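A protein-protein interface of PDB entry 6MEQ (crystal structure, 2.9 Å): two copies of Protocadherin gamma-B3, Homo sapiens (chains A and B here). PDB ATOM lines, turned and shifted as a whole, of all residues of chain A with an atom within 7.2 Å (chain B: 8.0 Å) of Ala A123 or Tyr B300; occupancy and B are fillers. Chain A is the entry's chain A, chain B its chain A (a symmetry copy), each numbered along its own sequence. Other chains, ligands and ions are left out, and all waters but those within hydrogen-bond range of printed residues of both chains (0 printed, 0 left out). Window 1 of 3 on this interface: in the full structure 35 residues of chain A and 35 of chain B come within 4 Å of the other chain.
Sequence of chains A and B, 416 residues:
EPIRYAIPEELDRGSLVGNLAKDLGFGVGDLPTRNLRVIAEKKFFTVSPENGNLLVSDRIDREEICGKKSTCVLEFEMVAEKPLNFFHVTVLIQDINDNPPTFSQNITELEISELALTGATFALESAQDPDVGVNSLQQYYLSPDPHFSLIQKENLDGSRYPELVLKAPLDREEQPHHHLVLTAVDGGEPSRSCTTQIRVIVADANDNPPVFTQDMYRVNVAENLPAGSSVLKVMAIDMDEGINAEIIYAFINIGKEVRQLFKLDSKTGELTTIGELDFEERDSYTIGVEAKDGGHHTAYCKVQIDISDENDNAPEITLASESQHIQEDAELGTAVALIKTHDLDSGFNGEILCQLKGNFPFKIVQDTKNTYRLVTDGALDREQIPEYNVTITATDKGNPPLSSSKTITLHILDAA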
ATOM      1  N   LEU A 110      36.795 -23.173 -13.329  1.00  0.00           N
ATOM      2  CA  LEU A 110      35.796 -23.130 -12.265  1.00  0.00           C
ATOM      3  C   LEU A 110      36.482 -22.658 -10.991  1.00  0.00           C
ATOM      4  O   LEU A 110      37.344 -23.361 -10.455  1.00  0.00           O
ATOM      5  CB  LEU A 110      35.148 -24.498 -12.069  1.00  0.00           C
ATOM      6  CG  LEU A 110      34.097 -24.614 -10.963  1.00  0.00           C
ATOM      7  CD1 LEU A 110      32.925 -23.682 -11.232  1.00  0.00           C
ATOM      8  CD2 LEU A 110      33.624 -26.054 -10.828  1.00  0.00           C
ATOM      9  N   THR A 121      28.582 -29.305  -3.674  1.00  0.00           N
ATOM     10  CA  THR A 121      28.276 -29.655  -5.052  1.00  0.00           C
ATOM     11  C   THR A 121      28.412 -28.425  -5.940  1.00  0.00           C
ATOM     12  O   THR A 121      27.989 -27.326  -5.565  1.00  0.00           O
ATOM     13  CB  THR A 121      26.862 -30.231  -5.169  1.00  0.00           C
ATOM     14  OG1 THR A 121      26.706 -31.307  -4.235  1.00  0.00           O
ATOM     15  CG2 THR A 121      26.611 -30.755  -6.574  1.00  0.00           C
ATOM     16  N   PHE A 122      29.008 -28.615  -7.115  1.00  0.00           N
ATOM     17  CA  PHE A 122      29.198 -27.546  -8.086  1.00  0.00           C
ATOM     18  C   PHE A 122      28.698 -28.020  -9.441  1.00  0.00           C
ATOM     19  O   PHE A 122      29.023 -29.132  -9.871  1.00  0.00           O
ATOM     20  CB  PHE A 122      30.669 -27.128  -8.164  1.00  0.00           C
ATOM     21  CG  PHE A 122      31.247 -26.713  -6.841  1.00  0.00           C
ATOM     22  CD1 PHE A 122      31.141 -25.403  -6.404  1.00  0.00           C
ATOM     23  CD2 PHE A 122      31.887 -27.636  -6.030  1.00  0.00           C
ATOM     24  CE1 PHE A 122      31.667 -25.019  -5.185  1.00  0.00           C
ATOM     25  CE2 PHE A 122      32.416 -27.259  -4.811  1.00  0.00           C
ATOM     26  CZ  PHE A 122      32.305 -25.949  -4.387  1.00  0.00           C
ATOM     27  N   ALA A 123      27.911 -27.179 -10.107  1.00  0.00           N
ATOM     28  CA  ALA A 123      27.273 -27.576 -11.354  1.00  0.00           C
ATOM     29  C   ALA A 123      28.289 -27.644 -12.486  1.00  0.00           C
ATOM     30  O   ALA A 123      29.121 -26.747 -12.649  1.00  0.00           O
ATOM     31  CB  ALA A 123      26.153 -26.598 -11.709  1.00  0.00           C
ATOM     32  N   LEU A 124      28.218 -28.717 -13.270  1.00  0.00           N
ATOM     33  CA  LEU A 124      29.042 -28.896 -14.454  1.00  0.00           C
ATOM     34  C   LEU A 124      28.167 -28.846 -15.699  1.00  0.00           C
ATOM     35  O   LEU A 124      27.002 -29.255 -15.677  1.00  0.00           O
ATOM     36  CB  LEU A 124      29.801 -30.226 -14.406  1.00  0.00           C
ATOM     37  CG  LEU A 124      30.784 -30.421 -13.252  1.00  0.00           C
ATOM     38  CD1 LEU A 124      31.412 -31.804 -13.316  1.00  0.00           C
ATOM     39  CD2 LEU A 124      31.854 -29.342 -13.270  1.00  0.00           C
ATOM     40  N   GLU A 125      28.739 -28.341 -16.788  1.00  0.00           N
ATOM     41  CA  GLU A 125      27.995 -28.239 -18.035  1.00  0.00           C
ATOM     42  C   GLU A 125      27.841 -29.611 -18.678  1.00  0.00           C
ATOM     43  O   GLU A 125      28.787 -30.403 -18.729  1.00  0.00           O
ATOM     44  CB  GLU A 125      28.696 -27.281 -18.997  1.00  0.00           C
ATOM     45  CG  GLU A 125      27.896 -26.972 -20.252  1.00  0.00           C
ATOM     46  CD  GLU A 125      28.544 -25.905 -21.110  1.00  0.00           C
ATOM     47  OE1 GLU A 125      29.763 -25.675 -20.957  1.00  0.00           O
ATOM     48  OE2 GLU A 125      27.833 -25.290 -21.932  1.00  0.00           O
ATOM     49  N   TYR A 161      22.771 -35.331 -16.181  1.00  0.00           N
ATOM     50  CA  TYR A 161      23.608 -34.144 -16.084  1.00  0.00           C
ATOM     51  C   TYR A 161      24.602 -34.364 -14.947  1.00  0.00           C
ATOM     52  O   TYR A 161      24.211 -34.846 -13.869  1.00  0.00           O
ATOM     53  CB  TYR A 161      22.789 -32.868 -15.849  1.00  0.00           C
ATOM     54  CG  TYR A 161      22.009 -32.835 -14.552  1.00  0.00           C
ATOM     55  CD1 TYR A 161      22.519 -32.197 -13.429  1.00  0.00           C
ATOM     56  CD2 TYR A 161      20.755 -33.427 -14.458  1.00  0.00           C
ATOM     57  CE1 TYR A 161      21.807 -32.158 -12.243  1.00  0.00           C
ATOM     58  CE2 TYR A 161      20.037 -33.392 -13.277  1.00  0.00           C
ATOM     59  CZ  TYR A 161      20.567 -32.756 -12.174  1.00  0.00           C
ATOM     60  OH  TYR A 161      19.854 -32.720 -10.996  1.00  0.00           O
ATOM     61  N   PRO A 162      25.876 -34.043 -15.152  1.00  0.00           N
ATOM     62  CA  PRO A 162      26.881 -34.264 -14.112  1.00  0.00           C
ATOM     63  C   PRO A 162      27.025 -33.069 -13.180  1.00  0.00           C
ATOM     64  O   PRO A 162      26.717 -31.926 -13.526  1.00  0.00           O
ATOM     65  CB  PRO A 162      28.166 -34.473 -14.925  1.00  0.00           C
ATOM     66  CG  PRO A 162      27.971 -33.585 -16.112  1.00  0.00           C
ATOM     67  CD  PRO A 162      26.483 -33.583 -16.415  1.00  0.00           C
ATOM     68  N   GLU A 163      27.507 -33.362 -11.974  1.00  0.00           N
ATOM     69  CA  GLU A 163      27.798 -32.338 -10.980  1.00  0.00           C
ATOM     70  C   GLU A 163      29.041 -32.738 -10.204  1.00  0.00           C
ATOM     71  O   GLU A 163      29.176 -33.895  -9.794  1.00  0.00           O
ATOM     72  CB  GLU A 163      26.616 -32.127 -10.024  1.00  0.00           C
ATOM     73  CG  GLU A 163      25.537 -31.203 -10.571  1.00  0.00           C
ATOM     74  CD  GLU A 163      24.469 -30.875  -9.546  1.00  0.00           C
ATOM     75  OE1 GLU A 163      24.263 -31.683  -8.617  1.00  0.00           O
ATOM     76  OE2 GLU A 163      23.837 -29.804  -9.668  1.00  0.00           O
ATOM     77  N   LEU A 164      29.944 -31.782 -10.009  1.00  0.00           N
ATOM     78  CA  LEU A 164      31.195 -32.040  -9.311  1.00  0.00           C
ATOM     79  C   LEU A 164      30.974 -31.984  -7.806  1.00  0.00           C
ATOM     80  O   LEU A 164      30.309 -31.075  -7.300  1.00  0.00           O
ATOM     81  CB  LEU A 164      32.253 -31.021  -9.736  1.00  0.00           C
ATOM     82  CG  LEU A 164      33.694 -31.274  -9.295  1.00  0.00           C
ATOM     83  CD1 LEU A 164      34.205 -32.584  -9.871  1.00  0.00           C
ATOM     84  CD2 LEU A 164      34.585 -30.116  -9.717  1.00  0.00           C
ATOM     85  N   PRO B 210      22.904 -15.628  -3.017  1.00  0.00           N
ATOM     86  CA  PRO B 210      21.790 -14.999  -3.736  1.00  0.00           C
ATOM     87  C   PRO B 210      20.551 -15.883  -3.728  1.00  0.00           C
ATOM     88  O   PRO B 210      20.635 -17.112  -3.721  1.00  0.00           O
ATOM     89  CB  PRO B 210      22.338 -14.818  -5.157  1.00  0.00           C
ATOM     90  CG  PRO B 210      23.823 -14.822  -4.993  1.00  0.00           C
ATOM     91  CD  PRO B 210      24.098 -15.770  -3.868  1.00  0.00           C
ATOM     92  N   VAL B 211      19.388 -15.235  -3.724  1.00  0.00           N
ATOM     93  CA  VAL B 211      18.099 -15.918  -3.692  1.00  0.00           C
ATOM     94  C   VAL B 211      17.204 -15.293  -4.753  1.00  0.00           C
ATOM     95  O   VAL B 211      16.957 -14.081  -4.726  1.00  0.00           O
ATOM     96  CB  VAL B 211      17.432 -15.833  -2.308  1.00  0.00           C
ATOM     97  CG1 VAL B 211      16.025 -16.407  -2.360  1.00  0.00           C
ATOM     98  CG2 VAL B 211      18.269 -16.560  -1.265  1.00  0.00           C
ATOM     99  N   PHE B 212      16.720 -16.115  -5.682  1.00  0.00           N
ATOM    100  CA  PHE B 212      15.797 -15.633  -6.698  1.00  0.00           C
ATOM    101  C   PHE B 212      14.412 -15.411  -6.103  1.00  0.00           C
ATOM    102  O   PHE B 212      14.000 -16.087  -5.155  1.00  0.00           O
ATOM    103  CB  PHE B 212      15.705 -16.626  -7.857  1.00  0.00           C
ATOM    104  CG  PHE B 212      16.896 -16.607  -8.773  1.00  0.00           C
ATOM    105  CD1 PHE B 212      17.001 -15.655  -9.774  1.00  0.00           C
ATOM    106  CD2 PHE B 212      17.903 -17.548  -8.643  1.00  0.00           C
ATOM    107  CE1 PHE B 212      18.092 -15.636 -10.622  1.00  0.00           C
ATOM    108  CE2 PHE B 212      18.997 -17.534  -9.488  1.00  0.00           C
ATOM    109  CZ  PHE B 212      19.091 -16.577 -10.479  1.00  0.00           C
ATOM    110  N   GLN B 214      11.618 -15.951  -7.759  1.00  0.00           N
ATOM    111  CA  GLN B 214      10.814 -17.069  -8.229  1.00  0.00           C
ATOM    112  C   GLN B 214      11.733 -18.177  -8.719  1.00  0.00           C
ATOM    113  O   GLN B 214      12.783 -17.909  -9.309  1.00  0.00           O
ATOM    114  CB  GLN B 214       9.867 -16.645  -9.359  1.00  0.00           C
ATOM    115  CG  GLN B 214       8.908 -15.525  -8.992  1.00  0.00           C
ATOM    116  CD  GLN B 214       8.058 -15.083 -10.168  1.00  0.00           C
ATOM    117  OE1 GLN B 214       8.142 -15.650 -11.256  1.00  0.00           O
ATOM    118  NE2 GLN B 214       7.236 -14.063  -9.953  1.00  0.00           N
ATOM    119  N   ASP B 215      11.333 -19.423  -8.470  1.00  0.00           N
ATOM    120  CA  ASP B 215      12.081 -20.575  -8.956  1.00  0.00           C
ATOM    121  C   ASP B 215      11.733 -20.941 -10.392  1.00  0.00           C
ATOM    122  O   ASP B 215      12.319 -21.885 -10.932  1.00  0.00           O
ATOM    123  CB  ASP B 215      11.842 -21.781  -8.043  1.00  0.00           C
ATOM    124  CG  ASP B 215      12.357 -21.559  -6.635  1.00  0.00           C
ATOM    125  OD1 ASP B 215      13.363 -20.836  -6.477  1.00  0.00           O
ATOM    126  OD2 ASP B 215      11.755 -22.105  -5.686  1.00  0.00           O
ATOM    127  N   MET B 216      10.805 -20.220 -11.018  1.00  0.00           N
ATOM    128  CA  MET B 216      10.399 -20.512 -12.390  1.00  0.00           C
ATOM    129  C   MET B 216       9.816 -19.247 -12.997  1.00  0.00           C
ATOM    130  O   MET B 216       8.790 -18.750 -12.521  1.00  0.00           O
ATOM    131  CB  MET B 216       9.379 -21.651 -12.430  1.00  0.00           C
ATOM    132  CG  MET B 216       8.805 -21.929 -13.811  1.00  0.00           C
ATOM    133  SD  MET B 216      10.039 -22.522 -14.982  1.00  0.00           S
ATOM    134  CE  MET B 216      10.539 -24.053 -14.201  1.00  0.00           C
ATOM    135  N   TYR B 217      10.466 -18.724 -14.034  1.00  0.00           N
ATOM    136  CA  TYR B 217       9.991 -17.545 -14.754  1.00  0.00           C
ATOM    137  C   TYR B 217       9.382 -18.016 -16.070  1.00  0.00           C
ATOM    138  O   TYR B 217      10.101 -18.335 -17.020  1.00  0.00           O
ATOM    139  CB  TYR B 217      11.125 -16.552 -14.984  1.00  0.00           C
ATOM    140  CG  TYR B 217      11.709 -15.976 -13.712  1.00  0.00           C
ATOM    141  CD1 TYR B 217      11.149 -14.856 -13.112  1.00  0.00           C
ATOM    142  CD2 TYR B 217      12.824 -16.551 -13.115  1.00  0.00           C
ATOM    143  CE1 TYR B 217      11.679 -14.326 -11.951  1.00  0.00           C
ATOM    144  CE2 TYR B 217      13.362 -16.028 -11.954  1.00  0.00           C
ATOM    145  CZ  TYR B 217      12.786 -14.916 -11.377  1.00  0.00           C
ATOM    146  OH  TYR B 217      13.318 -14.391 -10.221  1.00  0.00           O
ATOM    147  N   ALA B 250      24.011 -15.355 -15.788  1.00  0.00           N
ATOM    148  CA  ALA B 250      24.498 -16.058 -16.966  1.00  0.00           C
ATOM    149  C   ALA B 250      23.645 -17.302 -17.179  1.00  0.00           C
ATOM    150  O   ALA B 250      22.847 -17.688 -16.321  1.00  0.00           O
ATOM    151  CB  ALA B 250      25.980 -16.423 -16.830  1.00  0.00           C
ATOM    152  N   PHE B 251      23.827 -17.925 -18.339  1.00  0.00           N
ATOM    153  CA  PHE B 251      23.113 -19.138 -18.708  1.00  0.00           C
ATOM    154  C   PHE B 251      23.939 -20.374 -18.370  1.00  0.00           C
ATOM    155  O   PHE B 251      25.165 -20.319 -18.247  1.00  0.00           O
ATOM    156  CB  PHE B 251      22.771 -19.132 -20.201  1.00  0.00           C
ATOM    157  CG  PHE B 251      21.636 -18.216 -20.561  1.00  0.00           C
ATOM    158  CD1 PHE B 251      20.701 -17.841 -19.612  1.00  0.00           C
ATOM    159  CD2 PHE B 251      21.500 -17.734 -21.854  1.00  0.00           C
ATOM    160  CE1 PHE B 251      19.652 -17.003 -19.942  1.00  0.00           C
ATOM    161  CE2 PHE B 251      20.454 -16.894 -22.190  1.00  0.00           C
ATOM    162  CZ  PHE B 251      19.529 -16.529 -21.233  1.00  0.00           C
ATOM    163  N   ILE B 252      23.244 -21.501 -18.219  1.00  0.00           N
ATOM    164  CA  ILE B 252      23.874 -22.784 -17.932  1.00  0.00           C
ATOM    165  C   ILE B 252      23.224 -23.856 -18.797  1.00  0.00           C
ATOM    166  O   ILE B 252      22.021 -23.812 -19.074  1.00  0.00           O
ATOM    167  CB  ILE B 252      23.775 -23.167 -16.438  1.00  0.00           C
ATOM    168  CG1 ILE B 252      22.315 -23.173 -15.981  1.00  0.00           C
ATOM    169  CG2 ILE B 252      24.609 -22.224 -15.581  1.00  0.00           C
ATOM    170  CD1 ILE B 252      22.114 -23.704 -14.581  1.00  0.00           C
ATOM    171  N   ASN B 253      24.038 -24.823 -19.225  1.00  0.00           N
ATOM    172  CA  ASN B 253      23.584 -25.950 -20.041  1.00  0.00           C
ATOM    173  C   ASN B 253      22.829 -25.465 -21.278  1.00  0.00           C
ATOM    174  O   ASN B 253      21.760 -25.970 -21.626  1.00  0.00           O
ATOM    175  CB  ASN B 253      22.725 -26.911 -19.218  1.00  0.00           C
ATOM    176  CG  ASN B 253      23.473 -27.499 -18.038  1.00  0.00           C
ATOM    177  OD1 ASN B 253      24.681 -27.730 -18.108  1.00  0.00           O
ATOM    178  ND2 ASN B 253      22.759 -27.744 -16.946  1.00  0.00           N
ATOM    179  N   GLY B 288      18.262 -22.490 -17.981  1.00  0.00           N
ATOM    180  CA  GLY B 288      18.711 -22.347 -16.605  1.00  0.00           C
ATOM    181  C   GLY B 288      19.553 -21.094 -16.443  1.00  0.00           C
ATOM    182  O   GLY B 288      20.360 -20.758 -17.309  1.00  0.00           O
ATOM    183  N   VAL B 289      19.357 -20.407 -15.319  1.00  0.00           N
ATOM    184  CA  VAL B 289      20.036 -19.150 -15.026  1.00  0.00           C
ATOM    185  C   VAL B 289      20.841 -19.321 -13.746  1.00  0.00           C
ATOM    186  O   VAL B 289      20.338 -19.871 -12.759  1.00  0.00           O
ATOM    187  CB  VAL B 289      19.040 -17.984 -14.896  1.00  0.00           C
ATOM    188  CG1 VAL B 289      19.772 -16.687 -14.588  1.00  0.00           C
ATOM    189  CG2 VAL B 289      18.217 -17.847 -16.167  1.00  0.00           C
ATOM    190  N   GLU B 290      22.085 -18.851 -13.765  1.00  0.00           N
ATOM    191  CA  GLU B 290      22.978 -18.916 -12.617  1.00  0.00           C
ATOM    192  C   GLU B 290      23.235 -17.514 -12.081  1.00  0.00           C
ATOM    193  O   GLU B 290      23.445 -16.573 -12.853  1.00  0.00           O
ATOM    194  CB  GLU B 290      24.305 -19.583 -12.992  1.00  0.00           C
ATOM    195  CG  GLU B 290      25.309 -19.663 -11.853  1.00  0.00           C
ATOM    196  CD  GLU B 290      26.634 -20.259 -12.285  1.00  0.00           C
ATOM    197  OE1 GLU B 290      26.808 -20.512 -13.496  1.00  0.00           O
ATOM    198  OE2 GLU B 290      27.502 -20.476 -11.413  1.00  0.00           O
ATOM    199  N   ALA B 291      23.214 -17.381 -10.757  1.00  0.00           N
ATOM    200  CA  ALA B 291      23.474 -16.114 -10.082  1.00  0.00           C
ATOM    201  C   ALA B 291      24.713 -16.268  -9.214  1.00  0.00           C
ATOM    202  O   ALA B 291      24.738 -17.104  -8.304  1.00  0.00           O
ATOM    203  CB  ALA B 291      22.274 -15.680  -9.239  1.00  0.00           C
ATOM    204  N   LYS B 292      25.733 -15.463  -9.492  1.00  0.00           N
ATOM    205  CA  LYS B 292      27.005 -15.527  -8.792  1.00  0.00           C
ATOM    206  C   LYS B 292      27.279 -14.198  -8.100  1.00  0.00           C
ATOM    207  O   LYS B 292      26.869 -13.136  -8.577  1.00  0.00           O
ATOM    208  CB  LYS B 292      28.145 -15.858  -9.761  1.00  0.00           C
ATOM    209  CG  LYS B 292      29.074 -16.962  -9.295  1.00  0.00           C
ATOM    210  CD  LYS B 292      30.174 -17.199 -10.316  1.00  0.00           C
ATOM    211  CE  LYS B 292      31.319 -17.997  -9.721  1.00  0.00           C
ATOM    212  NZ  LYS B 292      32.633 -17.380 -10.054  1.00  0.00           N
ATOM    213  N   HIS B 296      31.573 -16.182  -4.601  1.00  0.00           N
ATOM    214  CA  HIS B 296      31.353 -17.354  -5.450  1.00  0.00           C
ATOM    215  C   HIS B 296      30.195 -18.216  -4.953  1.00  0.00           C
ATOM    216  O   HIS B 296      30.188 -19.435  -5.145  1.00  0.00           O
ATOM    217  CB  HIS B 296      32.628 -18.194  -5.578  1.00  0.00           C
ATOM    218  CG  HIS B 296      33.829 -17.405  -5.998  1.00  0.00           C
ATOM    219  ND1 HIS B 296      33.971 -16.882  -7.265  1.00  0.00           N
ATOM    220  CD2 HIS B 296      34.944 -17.048  -5.317  1.00  0.00           C
ATOM    221  CE1 HIS B 296      35.120 -16.237  -7.347  1.00  0.00           C
ATOM    222  NE2 HIS B 296      35.730 -16.324  -6.179  1.00  0.00           N
ATOM    223  N   HIS B 297      29.207 -17.595  -4.312  1.00  0.00           N
ATOM    224  CA  HIS B 297      27.990 -18.301  -3.935  1.00  0.00           C
ATOM    225  C   HIS B 297      27.047 -18.361  -5.129  1.00  0.00           C
ATOM    226  O   HIS B 297      26.756 -17.336  -5.755  1.00  0.00           O
ATOM    227  CB  HIS B 297      27.310 -17.614  -2.750  1.00  0.00           C
ATOM    228  CG  HIS B 297      27.925 -17.943  -1.425  1.00  0.00           C
ATOM    229  ND1 HIS B 297      29.028 -18.761  -1.300  1.00  0.00           N
ATOM    230  CD2 HIS B 297      27.590 -17.569  -0.169  1.00  0.00           C
ATOM    231  CE1 HIS B 297      29.347 -18.874  -0.022  1.00  0.00           C
ATOM    232  NE2 HIS B 297      28.489 -18.161   0.685  1.00  0.00           N
ATOM    233  N   THR B 298      26.574 -19.561  -5.446  1.00  0.00           N
ATOM    234  CA  THR B 298      25.771 -19.792  -6.636  1.00  0.00           C
ATOM    235  C   THR B 298      24.287 -19.858  -6.292  1.00  0.00           C
ATOM    236  O   THR B 298      23.901 -20.184  -5.167  1.00  0.00           O
ATOM    237  CB  THR B 298      26.194 -21.085  -7.336  1.00  0.00           C
ATOM    238  OG1 THR B 298      26.039 -22.190  -6.437  1.00  0.00           O
ATOM    239  CG2 THR B 298      27.647 -20.998  -7.781  1.00  0.00           C
ATOM    240  N   ALA B 299      23.461 -19.538  -7.285  1.00  0.00           N
ATOM    241  CA  ALA B 299      22.009 -19.623  -7.159  1.00  0.00           C
ATOM    242  C   ALA B 299      21.446 -19.959  -8.529  1.00  0.00           C
ATOM    243  O   ALA B 299      21.717 -19.246  -9.500  1.00  0.00           O
ATOM    244  CB  ALA B 299      21.417 -18.315  -6.632  1.00  0.00           C
ATOM    245  N   TYR B 300      20.669 -21.036  -8.609  1.00  0.00           N
ATOM    246  CA  TYR B 300      20.171 -21.544  -9.877  1.00  0.00           C
ATOM    247  C   TYR B 300      18.650 -21.504  -9.911  1.00  0.00           C
ATOM    248  O   TYR B 300      17.982 -21.630  -8.881  1.00  0.00           O
ATOM    249  CB  TYR B 300      20.654 -22.979 -10.126  1.00  0.00           C
ATOM    250  CG  TYR B 300      22.159 -23.134 -10.110  1.00  0.00           C
ATOM    251  CD1 TYR B 300      22.824 -23.522  -8.954  1.00  0.00           C
ATOM    252  CD2 TYR B 300      22.914 -22.892 -11.251  1.00  0.00           C
ATOM    253  CE1 TYR B 300      24.200 -23.665  -8.936  1.00  0.00           C
ATOM    254  CE2 TYR B 300      24.289 -23.033 -11.242  1.00  0.00           C
ATOM    255  CZ  TYR B 300      24.927 -23.419 -10.082  1.00  0.00           C
ATOM    256  OH  TYR B 300      26.296 -23.560 -10.068  1.00  0.00           O
ATOM    257  N   CYS B 301      18.112 -21.324 -11.115  1.00  0.00           N
ATOM    258  CA  CYS B 301      16.676 -21.373 -11.356  1.00  0.00           C
ATOM    259  C   CYS B 301      16.459 -21.812 -12.800  1.00  0.00           C
ATOM    260  O   CYS B 301      17.405 -22.176 -13.505  1.00  0.00           O
ATOM    261  CB  CYS B 301      16.021 -20.019 -11.053  1.00  0.00           C
ATOM    262  SG  CYS B 301      16.454 -18.693 -12.203  1.00  0.00           S
ATOM    263  N   LYS B 302      15.205 -21.781 -13.245  1.00  0.00           N
ATOM    264  CA  LYS B 302      14.855 -22.160 -14.604  1.00  0.00           C
ATOM    265  C   LYS B 302      13.913 -21.128 -15.204  1.00  0.00           C
ATOM    266  O   LYS B 302      13.085 -20.535 -14.506  1.00  0.00           O
ATOM    267  CB  LYS B 302      14.206 -23.552 -14.657  1.00  0.00           C
ATOM    268  CG  LYS B 302      15.161 -24.695 -14.348  1.00  0.00           C
ATOM    269  CD  LYS B 302      14.498 -26.046 -14.566  1.00  0.00           C
ATOM    270  CE  LYS B 302      15.473 -27.187 -14.319  1.00  0.00           C
ATOM    271  NZ  LYS B 302      14.846 -28.516 -14.559  1.00  0.00           N
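No position is printed for both chains. Of the 3 pairs that touch across the chains among the printed residues, none has its exchanged pair printed and touching as well.
Ala A123 touches just one residue of chain B: Tyr B300 (3.5 Å). Printed residues of chain B within 4 Å of Leu A124: Asn B253 (3.7 Å). Of the printed residues of chain B, Glu A125 touches Asn B253. Asp B215 touches none of the printed residues of chain A. Of the printed residues of chain A, Asn B253 touches Leu A124 (3.7 Å) and Glu A125 (3.4 Å). Of the printed residues of chain A, Tyr B300 touches Ala A123 (3.5 Å). The nearest residue of chain B that does not touch Ala A123 is Ile B252 (5.7 Å).
Among the printed residues, pairs that only touch across the chains: Glu A125 with Asn B253 (3.4 Å), Ala A123 with Tyr B300 (3.5 Å) and Leu A124 with Asn B253 (3.7 Å).
Of the 23 printed residues of chain B, 2 touch a printed residue of chain A. Hydrophobic or aromatic side chains of chain A within 4 Å of the printed part of chain B: Ala A123. Among the printed residues, no Asp or Glu carboxylate lies within 4 Å of a Lys or Arg side-chain nitrogen of the other chain.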
